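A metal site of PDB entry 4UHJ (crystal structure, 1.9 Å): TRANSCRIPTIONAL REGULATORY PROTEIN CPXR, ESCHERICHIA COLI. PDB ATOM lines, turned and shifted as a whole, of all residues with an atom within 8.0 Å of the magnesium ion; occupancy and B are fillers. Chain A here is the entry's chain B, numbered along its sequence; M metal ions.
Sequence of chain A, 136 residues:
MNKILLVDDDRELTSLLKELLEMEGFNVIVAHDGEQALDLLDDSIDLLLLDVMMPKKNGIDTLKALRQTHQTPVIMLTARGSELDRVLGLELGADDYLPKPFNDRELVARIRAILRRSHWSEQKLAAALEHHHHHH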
ATOM      1  N   VAL A   7      20.160 -19.002  14.308  1.00  0.00           N
ATOM      2  CA  VAL A   7      20.803 -20.172  14.928  1.00  0.00           C
ATOM      3  C   VAL A   7      21.970 -20.620  14.036  1.00  0.00           C
ATOM      4  O   VAL A   7      21.750 -21.100  12.946  1.00  0.00           O
ATOM      5  CB  VAL A   7      19.782 -21.345  15.154  1.00  0.00           C
ATOM      6  CG1 VAL A   7      20.409 -22.469  15.974  1.00  0.00           C
ATOM      7  CG2 VAL A   7      18.480 -20.849  15.783  1.00  0.00           C
ATOM      8  N   ASP A   8      23.192 -20.448  14.536  1.00  0.00           N
ATOM      9  CA  ASP A   8      24.429 -20.811  13.844  1.00  0.00           C
ATOM     10  C   ASP A   8      25.550 -20.861  14.877  1.00  0.00           C
ATOM     11  O   ASP A   8      25.617 -19.992  15.750  1.00  0.00           O
ATOM     12  CB  ASP A   8      24.731 -19.806  12.699  1.00  0.00           C
ATOM     13  CG  ASP A   8      25.770 -20.237  11.683  1.00  0.00           C
ATOM     14  OD1 ASP A   8      26.865 -20.695  12.095  1.00  0.00           O
ATOM     15  OD2 ASP A   8      25.492 -20.130  10.483  1.00  0.00           O
ATOM     16  N   ASP A   9      26.436 -21.859  14.777  1.00  0.00           N
ATOM     17  CA  ASP A   9      27.582 -22.031  15.688  1.00  0.00           C
ATOM     18  C   ASP A   9      28.741 -21.074  15.381  1.00  0.00           C
ATOM     19  O   ASP A   9      29.595 -20.868  16.242  1.00  0.00           O
ATOM     20  CB  ASP A   9      28.065 -23.483  15.660  1.00  0.00           C
ATOM     21  CG  ASP A   9      28.500 -23.968  14.276  1.00  0.00           C
ATOM     22  OD1 ASP A   9      27.671 -23.900  13.341  1.00  0.00           O
ATOM     23  OD2 ASP A   9      29.644 -24.456  14.151  1.00  0.00           O
ATOM     24  N   ASP A  10      28.778 -20.505  14.170  1.00  0.00           N
ATOM     25  CA  ASP A  10      29.826 -19.559  13.774  1.00  0.00           C
ATOM     26  C   ASP A  10      29.509 -18.184  14.380  1.00  0.00           C
ATOM     27  O   ASP A  10      28.676 -17.455  13.856  1.00  0.00           O
ATOM     28  CB  ASP A  10      29.946 -19.483  12.236  1.00  0.00           C
ATOM     29  CG  ASP A  10      31.079 -18.620  11.688  1.00  0.00           C
ATOM     30  OD1 ASP A  10      31.682 -17.858  12.470  1.00  0.00           O
ATOM     31  OD2 ASP A  10      31.331 -18.677  10.470  1.00  0.00           O
ATOM     32  N   LEU A  13      30.019 -15.185  11.996  1.00  0.00           N
ATOM     33  CA  LEU A  13      28.902 -15.025  11.074  1.00  0.00           C
ATOM     34  C   LEU A  13      27.656 -14.465  11.769  1.00  0.00           C
ATOM     35  O   LEU A  13      27.022 -13.560  11.214  1.00  0.00           O
ATOM     36  CB  LEU A  13      28.557 -16.329  10.346  1.00  0.00           C
ATOM     37  CG  LEU A  13      27.381 -16.275   9.346  1.00  0.00           C
ATOM     38  CD1 LEU A  13      27.605 -15.246   8.215  1.00  0.00           C
ATOM     39  CD2 LEU A  13      27.094 -17.638   8.779  1.00  0.00           C
ATOM     40  N   HIS A  32      23.596 -20.532  19.487  1.00  0.00           N
ATOM     41  CA  HIS A  32      24.795 -21.083  18.854  1.00  0.00           C
ATOM     42  C   HIS A  32      24.758 -22.598  18.645  1.00  0.00           C
ATOM     43  O   HIS A  32      25.714 -23.177  18.115  1.00  0.00           O
ATOM     44  CB  HIS A  32      26.043 -20.647  19.632  1.00  0.00           C
ATOM     45  CG  HIS A  32      26.252 -19.168  19.527  1.00  0.00           C
ATOM     46  ND1 HIS A  32      26.378 -18.563  18.280  1.00  0.00           N
ATOM     47  CD2 HIS A  32      26.316 -18.217  20.481  1.00  0.00           C
ATOM     48  CE1 HIS A  32      26.540 -17.267  18.532  1.00  0.00           C
ATOM     49  NE2 HIS A  32      26.510 -17.022  19.841  1.00  0.00           N
ATOM     50  N   ASP A  51      20.754 -22.919  10.980  1.00  0.00           N
ATOM     51  CA  ASP A  51      21.930 -23.535  10.362  1.00  0.00           C
ATOM     52  C   ASP A  51      21.777 -25.047  10.346  1.00  0.00           C
ATOM     53  O   ASP A  51      21.307 -25.623  11.329  1.00  0.00           O
ATOM     54  CB  ASP A  51      23.183 -23.176  11.145  1.00  0.00           C
ATOM     55  CG  ASP A  51      24.442 -23.351  10.341  1.00  0.00           C
ATOM     56  OD1 ASP A  51      24.380 -23.215   9.103  1.00  0.00           O
ATOM     57  OD2 ASP A  51      25.490 -23.598  10.955  1.00  0.00           O
ATOM     58  N   VAL A  52      22.128 -25.688   9.254  1.00  0.00           N
ATOM     59  CA  VAL A  52      21.976 -27.155   9.169  1.00  0.00           C
ATOM     60  C   VAL A  52      23.081 -27.855  10.006  1.00  0.00           C
ATOM     61  O   VAL A  52      22.783 -28.725  10.847  1.00  0.00           O
ATOM     62  CB  VAL A  52      21.948 -27.628   7.689  1.00  0.00           C
ATOM     63  CG1 VAL A  52      22.121 -29.153   7.561  1.00  0.00           C
ATOM     64  CG2 VAL A  52      20.670 -27.180   6.990  1.00  0.00           C
ATOM     65  N   MET A  53      24.337 -27.456   9.824  1.00  0.00           N
ATOM     66  CA  MET A  53      25.473 -28.134  10.446  1.00  0.00           C
ATOM     67  C   MET A  53      25.992 -27.404  11.707  1.00  0.00           C
ATOM     68  O   MET A  53      26.586 -26.324  11.609  1.00  0.00           O
ATOM     69  CB  MET A  53      26.555 -28.261   9.377  1.00  0.00           C
ATOM     70  CG  MET A  53      27.745 -29.045   9.763  1.00  0.00           C
ATOM     71  SD  MET A  53      28.454 -29.931   8.341  1.00  0.00           S
ATOM     72  CE  MET A  53      28.378 -28.620   6.936  1.00  0.00           C
ATOM     73  N   MET A  54      25.744 -28.011  12.893  1.00  0.00           N
ATOM     74  CA  MET A  54      26.121 -27.464  14.210  1.00  0.00           C
ATOM     75  C   MET A  54      26.495 -28.550  15.226  1.00  0.00           C
ATOM     76  O   MET A  54      25.931 -29.630  15.143  1.00  0.00           O
ATOM     77  CB  MET A  54      24.922 -26.661  14.832  1.00  0.00           C
ATOM     78  CG  MET A  54      24.455 -25.496  14.035  1.00  0.00           C
ATOM     79  SD  MET A  54      23.148 -24.647  14.912  1.00  0.00           S
ATOM     80  CE  MET A  54      21.754 -25.817  14.683  1.00  0.00           C
ATOM     81  N   PRO A  55      27.293 -28.254  16.289  1.00  0.00           N
ATOM     82  CA  PRO A  55      27.492 -29.239  17.369  1.00  0.00           C
ATOM     83  C   PRO A  55      26.278 -29.260  18.325  1.00  0.00           C
ATOM     84  O   PRO A  55      25.404 -28.376  18.257  1.00  0.00           O
ATOM     85  CB  PRO A  55      28.758 -28.743  18.067  1.00  0.00           C
ATOM     86  CG  PRO A  55      28.781 -27.287  17.846  1.00  0.00           C
ATOM     87  CD  PRO A  55      27.991 -26.985  16.591  1.00  0.00           C
ATOM     88  N   LEU A  77      19.819 -22.834   6.714  1.00  0.00           N
ATOM     89  CA  LEU A  77      21.047 -22.264   6.147  1.00  0.00           C
ATOM     90  C   LEU A  77      21.994 -23.408   5.815  1.00  0.00           C
ATOM     91  O   LEU A  77      22.231 -24.263   6.659  1.00  0.00           O
ATOM     92  CB  LEU A  77      21.722 -21.301   7.173  1.00  0.00           C
ATOM     93  CG  LEU A  77      20.775 -20.326   7.955  1.00  0.00           C
ATOM     94  CD1 LEU A  77      21.568 -19.497   8.952  1.00  0.00           C
ATOM     95  CD2 LEU A  77      19.974 -19.420   6.995  1.00  0.00           C
ATOM     96  N   THR A  78      22.541 -23.442   4.592  1.00  0.00           N
ATOM     97  CA  THR A  78      23.441 -24.563   4.282  1.00  0.00           C
ATOM     98  C   THR A  78      24.656 -24.070   3.500  1.00  0.00           C
ATOM     99  O   THR A  78      24.556 -23.134   2.719  1.00  0.00           O
ATOM    100  CB  THR A  78      22.686 -25.720   3.586  1.00  0.00           C
ATOM    101  OG1 THR A  78      23.510 -26.899   3.601  1.00  0.00           O
ATOM    102  CG2 THR A  78      22.189 -25.380   2.191  1.00  0.00           C
ATOM    103  N   ALA A  79      25.799 -24.691   3.750  1.00  0.00           N
ATOM    104  CA  ALA A  79      27.060 -24.339   3.092  1.00  0.00           C
ATOM    105  C   ALA A  79      27.005 -24.700   1.621  1.00  0.00           C
ATOM    106  O   ALA A  79      26.358 -25.681   1.249  1.00  0.00           O
ATOM    107  CB  ALA A  79      28.221 -25.053   3.760  1.00  0.00           C
ATOM    108  N   LYS A 100      25.046 -20.546   1.975  1.00  0.00           N
ATOM    109  CA  LYS A 100      26.135 -19.784   2.581  1.00  0.00           C
ATOM    110  C   LYS A 100      27.355 -19.841   1.630  1.00  0.00           C
ATOM    111  O   LYS A 100      27.643 -20.920   1.125  1.00  0.00           O
ATOM    112  CB  LYS A 100      26.461 -20.316   3.982  1.00  0.00           C
ATOM    113  CG  LYS A 100      25.320 -20.112   4.957  1.00  0.00           C
ATOM    114  CD  LYS A 100      25.742 -20.211   6.407  1.00  0.00           C
ATOM    115  CE  LYS A 100      25.852 -21.629   6.892  1.00  0.00           C
ATOM    116  NZ  LYS A 100      26.491 -21.685   8.242  1.00  0.00           N
HETATM  117 MG    MG M   1      27.503 -24.416  11.081  1.00  0.00          MG
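The backbone NH (N) of Asp 10 is in hydrogen-bond range of the side-chain carboxylate (OD1) of Asp 8 (2.8 Å). OD2 of Asp 8 lies within salt-bridge range of NZ of Lys 100 (2.9 Å). The side-chain carboxylate of Asp 51 lies within salt-bridge range of the side-chain amino group of Lys 100, at 2.7 Å. ND1 of His 32 lies within hydrogen-bond range of O of Asp 8, 3.0 Å away. The backbone carbonyl oxygen of Val 7 lies within hydrogen-bond range of the backbone NH of Asp 51, at 2.9 Å.
Asp 8 touches the magnesium ion. Within 4 Å of the magnesium ion: Asp 8, Asp 9, Asp 51 and Met 53. The nearest printed residue that does not touch the magnesium ion is Lys 100 (4.1 Å).
The magnesium ion is bound by OD2 of Asp 51 (2.2 Å), O of Met 53 (2.2 Å) and OD1 of Asp 9 (2.3 Å). The magnesium ion has three donor atoms within binding distance.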
